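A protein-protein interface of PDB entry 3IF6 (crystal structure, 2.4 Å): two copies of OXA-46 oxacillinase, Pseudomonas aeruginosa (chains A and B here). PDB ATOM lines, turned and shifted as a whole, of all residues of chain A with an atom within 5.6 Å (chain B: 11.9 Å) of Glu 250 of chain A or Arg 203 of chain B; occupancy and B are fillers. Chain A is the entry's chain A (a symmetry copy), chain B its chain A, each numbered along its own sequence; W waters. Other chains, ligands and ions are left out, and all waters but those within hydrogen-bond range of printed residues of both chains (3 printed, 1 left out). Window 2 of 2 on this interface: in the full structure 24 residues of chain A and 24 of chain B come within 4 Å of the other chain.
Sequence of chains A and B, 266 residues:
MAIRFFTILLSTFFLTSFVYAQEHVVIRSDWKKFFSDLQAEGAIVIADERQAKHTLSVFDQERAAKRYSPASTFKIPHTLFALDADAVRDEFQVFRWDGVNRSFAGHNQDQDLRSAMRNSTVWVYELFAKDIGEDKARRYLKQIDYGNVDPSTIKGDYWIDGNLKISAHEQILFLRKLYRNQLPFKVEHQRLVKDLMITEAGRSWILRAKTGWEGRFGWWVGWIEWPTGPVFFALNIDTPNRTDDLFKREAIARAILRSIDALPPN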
ATOM      1  N   ARG A 118     -10.591 -32.632 -11.148  1.00  0.00           N
ATOM      2  CA  ARG A 118      -9.665 -31.517 -10.968  1.00  0.00           C
ATOM      3  C   ARG A 118      -8.571 -31.808  -9.985  1.00  0.00           C
ATOM      4  O   ARG A 118      -7.562 -31.089  -9.965  1.00  0.00           O
ATOM      5  CB  ARG A 118     -10.381 -30.210 -10.583  1.00  0.00           C
ATOM      6  CG  ARG A 118     -11.267 -29.590 -11.667  1.00  0.00           C
ATOM      7  CD  ARG A 118     -12.181 -28.534 -11.049  1.00  0.00           C
ATOM      8  NE  ARG A 118     -12.830 -27.644 -12.012  1.00  0.00           N
ATOM      9  CZ  ARG A 118     -13.737 -26.704 -11.694  1.00  0.00           C
ATOM     10  NH1 ARG A 118     -14.153 -26.524 -10.414  1.00  0.00           N
ATOM     11  NH2 ARG A 118     -14.252 -25.930 -12.656  1.00  0.00           N
ATOM     12  N   ILE A 198     -12.627 -28.720 -18.855  1.00  0.00           N
ATOM     13  CA  ILE A 198     -12.343 -27.296 -18.934  1.00  0.00           C
ATOM     14  C   ILE A 198     -11.398 -26.832 -17.822  1.00  0.00           C
ATOM     15  O   ILE A 198     -11.702 -26.950 -16.630  1.00  0.00           O
ATOM     16  CB  ILE A 198     -13.631 -26.456 -18.898  1.00  0.00           C
ATOM     17  CG1 ILE A 198     -14.564 -26.898 -20.031  1.00  0.00           C
ATOM     18  CG2 ILE A 198     -13.283 -24.923 -18.936  1.00  0.00           C
ATOM     19  CD1 ILE A 198     -15.893 -26.168 -20.117  1.00  0.00           C
ATOM     20  N   THR A 199     -10.229 -26.329 -18.225  1.00  0.00           N
ATOM     21  CA  THR A 199      -9.302 -25.674 -17.281  1.00  0.00           C
ATOM     22  C   THR A 199      -9.337 -24.135 -17.422  1.00  0.00           C
ATOM     23  O   THR A 199      -8.921 -23.440 -16.524  1.00  0.00           O
ATOM     24  CB  THR A 199      -7.836 -26.235 -17.396  1.00  0.00           C
ATOM     25  OG1 THR A 199      -7.334 -26.033 -18.715  1.00  0.00           O
ATOM     26  CG2 THR A 199      -7.776 -27.762 -17.079  1.00  0.00           C
ATOM     27  N   GLU A 200      -9.861 -23.614 -18.531  1.00  0.00           N
ATOM     28  CA  GLU A 200      -9.741 -22.204 -18.839  1.00  0.00           C
ATOM     29  C   GLU A 200     -10.568 -21.827 -20.066  1.00  0.00           C
ATOM     30  O   GLU A 200     -10.798 -22.690 -20.947  1.00  0.00           O
ATOM     31  CB  GLU A 200      -8.270 -21.916 -19.138  1.00  0.00           C
ATOM     32  CG  GLU A 200      -7.833 -20.530 -18.816  1.00  0.00           C
ATOM     33  CD  GLU A 200      -6.307 -20.358 -18.884  1.00  0.00           C
ATOM     34  OE1 GLU A 200      -5.569 -21.354 -18.691  1.00  0.00           O
ATOM     35  OE2 GLU A 200      -5.856 -19.201 -19.104  1.00  0.00           O
ATOM     36  N   THR A 211      -3.543 -33.304 -17.126  1.00  0.00           N
ATOM     37  CA  THR A 211      -2.179 -33.768 -16.845  1.00  0.00           C
ATOM     38  C   THR A 211      -2.179 -35.238 -16.369  1.00  0.00           C
ATOM     39  O   THR A 211      -3.233 -35.810 -16.051  1.00  0.00           O
ATOM     40  CB  THR A 211      -1.445 -32.864 -15.803  1.00  0.00           C
ATOM     41  OG1 THR A 211      -2.055 -33.016 -14.522  1.00  0.00           O
ATOM     42  CG2 THR A 211      -1.480 -31.347 -16.171  1.00  0.00           C
ATOM     43  N   TRP A 220       0.695 -33.876 -20.717  1.00  0.00           N
ATOM     44  CA  TRP A 220      -0.404 -32.924 -20.747  1.00  0.00           C
ATOM     45  C   TRP A 220      -1.057 -33.153 -22.082  1.00  0.00           C
ATOM     46  O   TRP A 220      -0.354 -33.175 -23.090  1.00  0.00           O
ATOM     47  CB  TRP A 220       0.111 -31.499 -20.664  1.00  0.00           C
ATOM     48  CG  TRP A 220      -0.923 -30.528 -20.336  1.00  0.00           C
ATOM     49  CD1 TRP A 220      -1.838 -30.623 -19.326  1.00  0.00           C
ATOM     50  CD2 TRP A 220      -1.167 -29.272 -20.986  1.00  0.00           C
ATOM     51  NE1 TRP A 220      -2.679 -29.555 -19.363  1.00  0.00           N
ATOM     52  CE2 TRP A 220      -2.268 -28.678 -20.328  1.00  0.00           C
ATOM     53  CE3 TRP A 220      -0.555 -28.585 -22.048  1.00  0.00           C
ATOM     54  CZ2 TRP A 220      -2.781 -27.414 -20.693  1.00  0.00           C
ATOM     55  CZ3 TRP A 220      -1.084 -27.345 -22.441  1.00  0.00           C
ATOM     56  CH2 TRP A 220      -2.186 -26.773 -21.752  1.00  0.00           C
ATOM     57  N   LEU A 235       1.558 -34.052 -25.141  1.00  0.00           N
ATOM     58  CA  LEU A 235       2.942 -33.977 -24.766  1.00  0.00           C
ATOM     59  C   LEU A 235       3.177 -34.982 -23.650  1.00  0.00           C
ATOM     60  O   LEU A 235       2.347 -35.095 -22.767  1.00  0.00           O
ATOM     61  CB  LEU A 235       3.249 -32.546 -24.237  1.00  0.00           C
ATOM     62  CG  LEU A 235       4.575 -32.359 -23.479  1.00  0.00           C
ATOM     63  CD1 LEU A 235       5.238 -31.042 -23.798  1.00  0.00           C
ATOM     64  CD2 LEU A 235       4.525 -32.548 -21.948  1.00  0.00           C
ATOM     65  N   LEU A 246       7.450 -31.256 -13.040  1.00  0.00           N
ATOM     66  CA  LEU A 246       6.055 -31.281 -13.368  1.00  0.00           C
ATOM     67  C   LEU A 246       5.529 -30.003 -14.060  1.00  0.00           C
ATOM     68  O   LEU A 246       4.643 -30.061 -14.937  1.00  0.00           O
ATOM     69  CB  LEU A 246       5.282 -31.544 -12.097  1.00  0.00           C
ATOM     70  CG  LEU A 246       4.829 -32.932 -11.722  1.00  0.00           C
ATOM     71  CD1 LEU A 246       5.636 -34.018 -12.378  1.00  0.00           C
ATOM     72  CD2 LEU A 246       4.793 -33.075 -10.235  1.00  0.00           C
ATOM     73  N   PHE A 247       6.055 -28.853 -13.679  1.00  0.00           N
ATOM     74  CA  PHE A 247       5.612 -27.631 -14.284  1.00  0.00           C
ATOM     75  C   PHE A 247       5.946 -27.609 -15.783  1.00  0.00           C
ATOM     76  O   PHE A 247       5.233 -26.986 -16.565  1.00  0.00           O
ATOM     77  CB  PHE A 247       6.221 -26.423 -13.561  1.00  0.00           C
ATOM     78  CG  PHE A 247       7.636 -26.082 -14.020  1.00  0.00           C
ATOM     79  CD1 PHE A 247       7.851 -25.187 -15.067  1.00  0.00           C
ATOM     80  CD2 PHE A 247       8.742 -26.682 -13.423  1.00  0.00           C
ATOM     81  CE1 PHE A 247       9.164 -24.907 -15.478  1.00  0.00           C
ATOM     82  CE2 PHE A 247      10.002 -26.416 -13.836  1.00  0.00           C
ATOM     83  CZ  PHE A 247      10.226 -25.507 -14.852  1.00  0.00           C
ATOM     84  N   KCX A 248       7.022 -28.299 -16.187  1.00  0.00           N
ATOM     85  CA  KCX A 248       7.448 -28.331 -17.616  1.00  0.00           C
ATOM     86  CB  KCX A 248       8.792 -29.045 -17.787  1.00  0.00           C
ATOM     87  CG  KCX A 248       9.896 -28.568 -16.813  1.00  0.00           C
ATOM     88  CD  KCX A 248      11.231 -29.255 -17.087  1.00  0.00           C
ATOM     89  CE  KCX A 248      12.110 -29.304 -15.854  1.00  0.00           C
ATOM     90  NZ  KCX A 248      13.515 -28.931 -16.106  1.00  0.00           N
ATOM     91  C   KCX A 248       6.409 -28.935 -18.558  1.00  0.00           C
ATOM     92  O   KCX A 248       6.384 -28.578 -19.745  1.00  0.00           O
ATOM     93  CX  KCX A 248      14.423 -28.709 -15.114  1.00  0.00           C
ATOM     94  OQ1 KCX A 248      15.620 -28.348 -15.392  1.00  0.00           O
ATOM     95  OQ2 KCX A 248      14.097 -28.863 -13.899  1.00  0.00           O
ATOM     96  N   ARG A 249       5.521 -29.800 -18.048  1.00  0.00           N
ATOM     97  CA  ARG A 249       4.475 -30.381 -18.892  1.00  0.00           C
ATOM     98  C   ARG A 249       3.671 -29.323 -19.616  1.00  0.00           C
ATOM     99  O   ARG A 249       3.720 -29.268 -20.838  1.00  0.00           O
ATOM    100  CB  ARG A 249       3.557 -31.337 -18.130  1.00  0.00           C
ATOM    101  CG  ARG A 249       4.301 -32.515 -17.518  1.00  0.00           C
ATOM    102  CD  ARG A 249       3.447 -33.233 -16.520  1.00  0.00           C
ATOM    103  NE  ARG A 249       2.995 -32.340 -15.466  1.00  0.00           N
ATOM    104  CZ  ARG A 249       2.130 -32.680 -14.512  1.00  0.00           C
ATOM    105  NH1 ARG A 249       1.643 -33.919 -14.453  1.00  0.00           N
ATOM    106  NH2 ARG A 249       1.773 -31.785 -13.592  1.00  0.00           N
ATOM    107  N   GLU A 250       2.922 -28.506 -18.870  1.00  0.00           N
ATOM    108  CA  GLU A 250       2.169 -27.376 -19.408  1.00  0.00           C
ATOM    109  C   GLU A 250       3.039 -26.272 -19.960  1.00  0.00           C
ATOM    110  O   GLU A 250       2.645 -25.632 -20.938  1.00  0.00           O
ATOM    111  CB  GLU A 250       1.277 -26.744 -18.334  1.00  0.00           C
ATOM    112  CG  GLU A 250      -0.061 -27.272 -18.355  1.00  0.00           C
ATOM    113  CD  GLU A 250      -1.044 -26.532 -17.510  1.00  0.00           C
ATOM    114  OE1 GLU A 250      -1.513 -25.407 -17.873  1.00  0.00           O
ATOM    115  OE2 GLU A 250      -1.381 -27.125 -16.481  1.00  0.00           O
ATOM    116  N   ALA A 251       4.174 -26.002 -19.319  1.00  0.00           N
ATOM    117  CA  ALA A 251       5.030 -24.903 -19.757  1.00  0.00           C
ATOM    118  C   ALA A 251       5.511 -25.067 -21.197  1.00  0.00           C
ATOM    119  O   ALA A 251       5.376 -24.134 -22.001  1.00  0.00           O
ATOM    120  CB  ALA A 251       6.209 -24.676 -18.783  1.00  0.00           C
ATOM    121  N   ILE A 252       6.033 -26.256 -21.533  1.00  0.00           N
ATOM    122  CA  ILE A 252       6.555 -26.514 -22.880  1.00  0.00           C
ATOM    123  C   ILE A 252       5.418 -26.472 -23.890  1.00  0.00           C
ATOM    124  O   ILE A 252       5.498 -25.759 -24.909  1.00  0.00           O
ATOM    125  CB  ILE A 252       7.388 -27.825 -22.964  1.00  0.00           C
ATOM    126  CG1 ILE A 252       8.644 -27.710 -22.122  1.00  0.00           C
ATOM    127  CG2 ILE A 252       7.826 -28.085 -24.392  1.00  0.00           C
ATOM    128  CD1 ILE A 252       9.205 -29.037 -21.637  1.00  0.00           C
ATOM    129  N   ALA A 253       4.327 -27.177 -23.590  1.00  0.00           N
ATOM    130  CA  ALA A 253       3.197 -27.202 -24.501  1.00  0.00           C
ATOM    131  C   ALA A 253       2.651 -25.820 -24.764  1.00  0.00           C
ATOM    132  O   ALA A 253       2.343 -25.476 -25.914  1.00  0.00           O
ATOM    133  CB  ALA A 253       2.105 -28.139 -24.003  1.00  0.00           C
ATOM    134  N   ARG A 254       2.495 -25.027 -23.703  1.00  0.00           N
ATOM    135  CA  ARG A 254       2.019 -23.652 -23.842  1.00  0.00           C
ATOM    136  C   ARG A 254       2.926 -22.760 -24.695  1.00  0.00           C
ATOM    137  O   ARG A 254       2.420 -21.987 -25.516  1.00  0.00           O
ATOM    138  CB  ARG A 254       1.764 -23.033 -22.465  1.00  0.00           C
ATOM    139  CG  ARG A 254       0.459 -23.549 -21.771  1.00  0.00           C
ATOM    140  CD  ARG A 254       0.323 -22.927 -20.360  1.00  0.00           C
ATOM    141  NE  ARG A 254      -0.999 -23.159 -19.814  1.00  0.00           N
ATOM    142  CZ  ARG A 254      -2.032 -22.322 -19.919  1.00  0.00           C
ATOM    143  NH1 ARG A 254      -1.882 -21.146 -20.501  1.00  0.00           N
ATOM    144  NH2 ARG A 254      -3.210 -22.672 -19.413  1.00  0.00           N
ATOM    145  N   ALA A 255       4.255 -22.876 -24.544  1.00  0.00           N
ATOM    146  CA  ALA A 255       5.174 -22.087 -25.371  1.00  0.00           C
ATOM    147  C   ALA A 255       4.968 -22.436 -26.833  1.00  0.00           C
ATOM    148  O   ALA A 255       4.887 -21.530 -27.678  1.00  0.00           O
ATOM    149  CB  ALA A 255       6.606 -22.308 -24.964  1.00  0.00           C
ATOM    150  N   ILE B 198     -20.637 -20.657 -22.224  1.00  0.00           N
ATOM    151  CA  ILE B 198     -19.359 -20.311 -21.622  1.00  0.00           C
ATOM    152  C   ILE B 198     -18.766 -19.031 -22.219  1.00  0.00           C
ATOM    153  O   ILE B 198     -18.495 -18.951 -23.422  1.00  0.00           O
ATOM    154  CB  ILE B 198     -18.342 -21.457 -21.748  1.00  0.00           C
ATOM    155  CG1 ILE B 198     -18.922 -22.731 -21.122  1.00  0.00           C
ATOM    156  CG2 ILE B 198     -16.960 -21.030 -21.132  1.00  0.00           C
ATOM    157  CD1 ILE B 198     -18.036 -23.962 -21.183  1.00  0.00           C
ATOM    158  N   GLU B 200     -16.175 -17.571 -20.128  1.00  0.00           N
ATOM    159  CA  GLU B 200     -14.947 -17.454 -19.370  1.00  0.00           C
ATOM    160  C   GLU B 200     -14.796 -18.597 -18.369  1.00  0.00           C
ATOM    161  O   GLU B 200     -15.820 -19.155 -17.908  1.00  0.00           O
ATOM    162  CB  GLU B 200     -15.001 -16.136 -18.596  1.00  0.00           C
ATOM    163  CG  GLU B 200     -13.673 -15.521 -18.328  1.00  0.00           C
ATOM    164  CD  GLU B 200     -13.782 -14.087 -17.786  1.00  0.00           C
ATOM    165  OE1 GLU B 200     -14.792 -13.400 -18.070  1.00  0.00           O
ATOM    166  OE2 GLU B 200     -12.823 -13.647 -17.093  1.00  0.00           O
ATOM    167  N   ALA B 201     -13.553 -18.953 -18.009  1.00  0.00           N
ATOM    168  CA  ALA B 201     -13.303 -20.034 -16.987  1.00  0.00           C
ATOM    169  C   ALA B 201     -11.876 -20.010 -16.502  1.00  0.00           C
ATOM    170  O   ALA B 201     -11.010 -19.501 -17.193  1.00  0.00           O
ATOM    171  CB  ALA B 201     -13.611 -21.427 -17.552  1.00  0.00           C
ATOM    172  N   GLY B 202     -11.652 -20.591 -15.330  1.00  0.00           N
ATOM    173  CA  GLY B 202     -10.344 -20.738 -14.704  1.00  0.00           C
ATOM    174  C   GLY B 202     -10.333 -22.154 -14.175  1.00  0.00           C
ATOM    175  O   GLY B 202     -11.247 -22.925 -14.515  1.00  0.00           O
ATOM    176  N   ARG B 203      -9.338 -22.513 -13.352  1.00  0.00           N
ATOM    177  CA  ARG B 203      -9.195 -23.886 -12.799  1.00  0.00           C
ATOM    178  C   ARG B 203     -10.421 -24.355 -12.026  1.00  0.00           C
ATOM    179  O   ARG B 203     -10.797 -25.543 -12.059  1.00  0.00           O
ATOM    180  CB  ARG B 203      -7.993 -23.948 -11.818  1.00  0.00           C
ATOM    181  CG  ARG B 203      -6.684 -24.562 -12.347  1.00  0.00           C
ATOM    182  CD  ARG B 203      -6.448 -24.195 -13.804  1.00  0.00           C
ATOM    183  NE  ARG B 203      -5.048 -24.192 -14.213  1.00  0.00           N
ATOM    184  CZ  ARG B 203      -4.305 -25.276 -14.449  1.00  0.00           C
ATOM    185  NH1 ARG B 203      -4.816 -26.492 -14.261  1.00  0.00           N
ATOM    186  NH2 ARG B 203      -3.033 -25.134 -14.866  1.00  0.00           N
ATOM    187  N   SER B 204     -11.021 -23.397 -11.331  1.00  0.00           N
ATOM    188  CA  SER B 204     -11.991 -23.637 -10.274  1.00  0.00           C
ATOM    189  C   SER B 204     -13.381 -23.217 -10.608  1.00  0.00           C
ATOM    190  O   SER B 204     -14.286 -23.518  -9.850  1.00  0.00           O
ATOM    191  CB  SER B 204     -11.628 -22.765  -9.078  1.00  0.00           C
ATOM    192  OG  SER B 204     -10.711 -23.454  -8.257  1.00  0.00           O
ATOM    193  N   TRP B 205     -13.546 -22.460 -11.688  1.00  0.00           N
ATOM    194  CA  TRP B 205     -14.770 -21.784 -11.960  1.00  0.00           C
ATOM    195  C   TRP B 205     -15.075 -21.684 -13.436  1.00  0.00           C
ATOM    196  O   TRP B 205     -14.170 -21.580 -14.270  1.00  0.00           O
ATOM    197  CB  TRP B 205     -14.750 -20.382 -11.351  1.00  0.00           C
ATOM    198  CG  TRP B 205     -13.633 -19.555 -11.842  1.00  0.00           C
ATOM    199  CD1 TRP B 205     -12.372 -19.518 -11.344  1.00  0.00           C
ATOM    200  CD2 TRP B 205     -13.683 -18.610 -12.918  1.00  0.00           C
ATOM    201  NE1 TRP B 205     -11.610 -18.640 -12.069  1.00  0.00           N
ATOM    202  CE2 TRP B 205     -12.387 -18.070 -13.049  1.00  0.00           C
ATOM    203  CE3 TRP B 205     -14.694 -18.194 -13.808  1.00  0.00           C
ATOM    204  CZ2 TRP B 205     -12.063 -17.119 -14.014  1.00  0.00           C
ATOM    205  CZ3 TRP B 205     -14.394 -17.239 -14.758  1.00  0.00           C
ATOM    206  CH2 TRP B 205     -13.058 -16.713 -14.858  1.00  0.00           C
ATOM    207  N   ILE B 206     -16.376 -21.708 -13.732  1.00  0.00           N
ATOM    208  CA  ILE B 206     -16.892 -21.549 -15.098  1.00  0.00           C
ATOM    209  C   ILE B 206     -17.983 -20.515 -15.121  1.00  0.00           C
ATOM    210  O   ILE B 206     -18.980 -20.659 -14.398  1.00  0.00           O
ATOM    211  CB  ILE B 206     -17.418 -22.895 -15.693  1.00  0.00           C
ATOM    212  CG1 ILE B 206     -16.351 -24.001 -15.559  1.00  0.00           C
ATOM    213  CG2 ILE B 206     -17.819 -22.721 -17.134  1.00  0.00           C
ATOM    214  CD1 ILE B 206     -16.783 -25.332 -16.184  1.00  0.00           C
ATOM    215  N   LEU B 207     -17.828 -19.501 -15.979  1.00  0.00           N
ATOM    216  CA  LEU B 207     -18.837 -18.489 -16.151  1.00  0.00           C
ATOM    217  C   LEU B 207     -19.618 -18.788 -17.421  1.00  0.00           C
ATOM    218  O   LEU B 207     -19.007 -18.953 -18.474  1.00  0.00           O
ATOM    219  CB  LEU B 207     -18.180 -17.091 -16.166  1.00  0.00           C
ATOM    220  CG  LEU B 207     -18.967 -15.887 -16.646  1.00  0.00           C
ATOM    221  CD1 LEU B 207     -20.203 -15.780 -15.814  1.00  0.00           C
ATOM    222  CD2 LEU B 207     -18.143 -14.651 -16.510  1.00  0.00           C
ATOM    223  N   ARG B 208     -20.955 -18.895 -17.325  1.00  0.00           N
ATOM    224  CA  ARG B 208     -21.838 -19.248 -18.477  1.00  0.00           C
ATOM    225  C   ARG B 208     -22.930 -18.178 -18.517  1.00  0.00           C
ATOM    226  O   ARG B 208     -23.713 -18.103 -17.575  1.00  0.00           O
ATOM    227  CB  ARG B 208     -22.479 -20.661 -18.324  1.00  0.00           C
ATOM    228  CG  ARG B 208     -21.599 -21.689 -17.684  1.00  0.00           C
ATOM    229  CD  ARG B 208     -22.216 -23.108 -17.408  1.00  0.00           C
ATOM    230  NE  ARG B 208     -21.678 -23.958 -18.432  1.00  0.00           N
ATOM    231  CZ  ARG B 208     -20.919 -25.038 -18.329  1.00  0.00           C
ATOM    232  NH1 ARG B 208     -20.613 -25.636 -17.171  1.00  0.00           N
ATOM    233  NH2 ARG B 208     -20.502 -25.562 -19.490  1.00  0.00           N
ATOM    234  N   ILE B 224     -22.133 -18.480 -12.522  1.00  0.00           N
ATOM    235  CA  ILE B 224     -20.758 -18.914 -12.373  1.00  0.00           C
ATOM    236  C   ILE B 224     -20.754 -20.099 -11.372  1.00  0.00           C
ATOM    237  O   ILE B 224     -21.388 -20.024 -10.304  1.00  0.00           O
ATOM    238  CB  ILE B 224     -19.863 -17.736 -11.898  1.00  0.00           C
ATOM    239  CG1 ILE B 224     -18.396 -18.177 -11.815  1.00  0.00           C
ATOM    240  CG2 ILE B 224     -20.421 -17.098 -10.588  1.00  0.00           C
ATOM    241  CD1 ILE B 224     -17.393 -17.039 -11.986  1.00  0.00           C
ATOM    242  N   GLU B 225     -20.081 -21.195 -11.744  1.00  0.00           N
ATOM    243  CA  GLU B 225     -19.967 -22.385 -10.915  1.00  0.00           C
ATOM    244  C   GLU B 225     -18.674 -22.365 -10.148  1.00  0.00           C
ATOM    245  O   GLU B 225     -17.654 -22.003 -10.707  1.00  0.00           O
ATOM    246  CB  GLU B 225     -19.937 -23.604 -11.792  1.00  0.00           C
ATOM    247  CG  GLU B 225     -21.131 -23.699 -12.704  1.00  0.00           C
ATOM    248  CD  GLU B 225     -21.077 -24.871 -13.644  1.00  0.00           C
ATOM    249  OE1 GLU B 225     -20.154 -25.691 -13.581  1.00  0.00           O
ATOM    250  OE2 GLU B 225     -22.000 -24.969 -14.440  1.00  0.00           O
ATOM    251  N   TRP B 226     -18.718 -22.783  -8.880  1.00  0.00           N
ATOM    252  CA  TRP B 226     -17.541 -22.841  -8.019  1.00  0.00           C
ATOM    253  C   TRP B 226     -17.558 -24.246  -7.499  1.00  0.00           C
ATOM    254  O   TRP B 226     -18.570 -24.868  -7.649  1.00  0.00           O
ATOM    255  CB  TRP B 226     -17.656 -21.781  -6.925  1.00  0.00           C
ATOM    256  CG  TRP B 226     -17.348 -20.391  -7.450  1.00  0.00           C
ATOM    257  CD1 TRP B 226     -18.247 -19.436  -7.820  1.00  0.00           C
ATOM    258  CD2 TRP B 226     -16.035 -19.840  -7.707  1.00  0.00           C
ATOM    259  NE1 TRP B 226     -17.581 -18.320  -8.279  1.00  0.00           N
ATOM    260  CE2 TRP B 226     -16.223 -18.530  -8.195  1.00  0.00           C
ATOM    261  CE3 TRP B 226     -14.719 -20.325  -7.534  1.00  0.00           C
ATOM    262  CZ2 TRP B 226     -15.142 -17.674  -8.541  1.00  0.00           C
ATOM    263  CZ3 TRP B 226     -13.610 -19.453  -7.876  1.00  0.00           C
ATOM    264  CH2 TRP B 226     -13.856 -18.148  -8.392  1.00  0.00           C
ATOM    265  N   PRO B 227     -16.454 -24.787  -6.945  1.00  0.00           N
ATOM    266  CA  PRO B 227     -16.563 -26.195  -6.437  1.00  0.00           C
ATOM    267  C   PRO B 227     -17.768 -26.554  -5.513  1.00  0.00           C
ATOM    268  O   PRO B 227     -18.236 -27.711  -5.469  1.00  0.00           O
ATOM    269  CB  PRO B 227     -15.243 -26.396  -5.692  1.00  0.00           C
ATOM    270  CG  PRO B 227     -14.292 -25.516  -6.401  1.00  0.00           C
ATOM    271  CD  PRO B 227     -15.080 -24.270  -6.782  1.00  0.00           C
ATOM    272  N   THR B 228     -18.260 -25.561  -4.790  1.00  0.00           N
ATOM    273  CA  THR B 228     -19.330 -25.757  -3.828  1.00  0.00           C
ATOM    274  C   THR B 228     -20.730 -25.437  -4.381  1.00  0.00           C
ATOM    275  O   THR B 228     -21.749 -25.727  -3.742  1.00  0.00           O
ATOM    276  CB  THR B 228     -19.018 -24.950  -2.594  1.00  0.00           C
ATOM    277  OG1 THR B 228     -18.292 -23.762  -2.984  1.00  0.00           O
ATOM    278  CG2 THR B 228     -18.100 -25.797  -1.688  1.00  0.00           C
ATOM    279  N   LEU B 263     -16.732 -13.917  -8.184  1.00  0.00           N
ATOM    280  CA  LEU B 263     -15.837 -13.724  -9.298  1.00  0.00           C
ATOM    281  C   LEU B 263     -14.420 -13.615  -8.753  1.00  0.00           C
ATOM    282  O   LEU B 263     -14.247 -13.138  -7.643  1.00  0.00           O
ATOM    283  CB  LEU B 263     -16.134 -12.398 -10.004  1.00  0.00           C
ATOM    284  CG  LEU B 263     -17.104 -12.239 -11.170  1.00  0.00           C
ATOM    285  CD1 LEU B 263     -16.850 -10.862 -11.724  1.00  0.00           C
ATOM    286  CD2 LEU B 263     -16.930 -13.304 -12.239  1.00  0.00           C
ATOM    287  N   PRO B 264     -13.406 -14.033  -9.537  1.00  0.00           N
ATOM    288  CA  PRO B 264     -12.004 -13.755  -9.146  1.00  0.00           C
ATOM    289  C   PRO B 264     -11.641 -12.254  -9.201  1.00  0.00           C
ATOM    290  O   PRO B 264     -12.198 -11.517 -10.025  1.00  0.00           O
ATOM    291  CB  PRO B 264     -11.168 -14.563 -10.159  1.00  0.00           C
ATOM    292  CG  PRO B 264     -12.121 -15.465 -10.825  1.00  0.00           C
ATOM    293  CD  PRO B 264     -13.472 -14.780 -10.807  1.00  0.00           C
ATOM    294  N   PRO B 265     -10.768 -11.798  -8.273  1.00  0.00           N
ATOM    295  CA  PRO B 265     -10.254 -10.421  -8.072  1.00  0.00           C
ATOM    296  C   PRO B 265      -9.981  -9.485  -9.281  1.00  0.00           C
ATOM    297  O   PRO B 265     -10.196  -8.274  -9.139  1.00  0.00           O
ATOM    298  CB  PRO B 265      -8.959 -10.633  -7.258  1.00  0.00           C
ATOM    299  CG  PRO B 265      -8.971 -12.075  -6.784  1.00  0.00           C
ATOM    300  CD  PRO B 265     -10.283 -12.693  -7.202  1.00  0.00           C
HETATM  301  O   HOH W   1      -6.416 -22.766 -16.451  1.00  0.00           O
HETATM  302  O   HOH W   2     -12.923 -24.982 -14.817  1.00  0.00           O
HETATM  303  O   HOH W   3     -16.354 -25.301 -11.145  1.00  0.00           O
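The guanidinium group of Arg 118 of chain A sits at hydrogen-bond distance from the backbone carbonyl oxygen of Arg 203 of chain B (2.9 Å).
The backbone NH (N) of Arg 203 of chain B is in hydrogen-bond range of the backbone carbonyl oxygen (O) of Thr 199 of chain A (3.3 Å).
NH2 of Arg 203 of chain B lies within salt-bridge range of OE2 of Glu 250 of chain A.
The backbone carbonyl oxygen (O) of Ser 204 of chain B is in hydrogen-bond range of the guanidinium group (NH1) of Arg 118 of chain A (3.1 Å).
The backbone carbonyl oxygen (O) of Gly 202 of chain B lies close to the backbone carbonyl oxygen (O) of Thr 199 of chain A.
NH2 of Arg 254 of chain A is in salt-bridge range of OE1 of Glu 200 of chain A (2.8 Å).
OE1 of Glu 250 of chain A lies within salt-bridge range of NE of Arg 254 of chain A.
N of Trp 205 of chain B touches NH2 of Arg 118 of chain A, at 3.7 Å.
CD1 of Ile 198 of chain A touches CD1 of Ile 198 of chain B (3.3 Å).
CB of Ala 201 of chain B touches CG2 of Ile 198 of chain A (3.8 Å).
Glu 200 of chain A touches Ala 201 of chain B.
Arg 118 of chain A touches just these residues of chain B: Arg 203, Ser 204 and Trp 205.
Of chain B, only Gly 202 (3.0 Å) and Arg 203 (3.3 Å) come within 4 Å of Thr 199 of chain A.
No residue of chain B comes within 4 Å of Trp 220 of chain A.
No residue of chain B comes within 4 Å of Arg 254 of chain A.
Of the printed residues of chain A, Ser 204 of chain B touches Arg 118.
Of the printed residues of chain B, Ile 198 of chain A touches Ile 198 and Ala 201.
Of the printed residues of chain A, Ala 201 of chain B touches Ile 198 and Glu 200.
Ile 206 of chain B touches none of the printed residues of chain A.
The nearest printed residue of chain A that does not touch Trp 205 of chain B is Ile 198 of chain A (5.8 Å).
Of the 18 printed residues of chain B, 6 touch a printed residue of chain A.
Printed residues of chain B that touch a printed residue of chain A: Ile 198, Ala 201, Gly 202, Arg 203, Ser 204 and Trp 205.
Hydrophobic or aromatic side chains of chain B within 4 Å of the printed part of chain A: Ile 198 and Ala 201.
Printed residues of chain A that touch a printed residue of chain B: Arg 118, Ile 198, Thr 199, Glu 200 and Glu 250.
Along chain A the printed residues that touch a printed residue of chain B span positions 118 to 250.
Among the printed residues, Asp or Glu carboxylates within 4 Å of a Lys or Arg side-chain nitrogen of the other chain: Glu 250 of chain A with Arg 203 of chain B (3.0 Å).
Ile 198 of chain A touches its own counterpart, Ile 198 of chain B.
Of the 9 pairs that touch across the chains among the printed residues, 1 has its exchanged pair printed and touching as well.
Water W2 lies within hydrogen-bond range of the backbone carbonyl oxygen (O) of Gly 202 of chain B (2.7 Å), the guanidinium group (NH2) of Arg 118 of chain A (2.7 Å) and the backbone carbonyl oxygen (O) of Ile 198 of chain A (2.9 Å).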
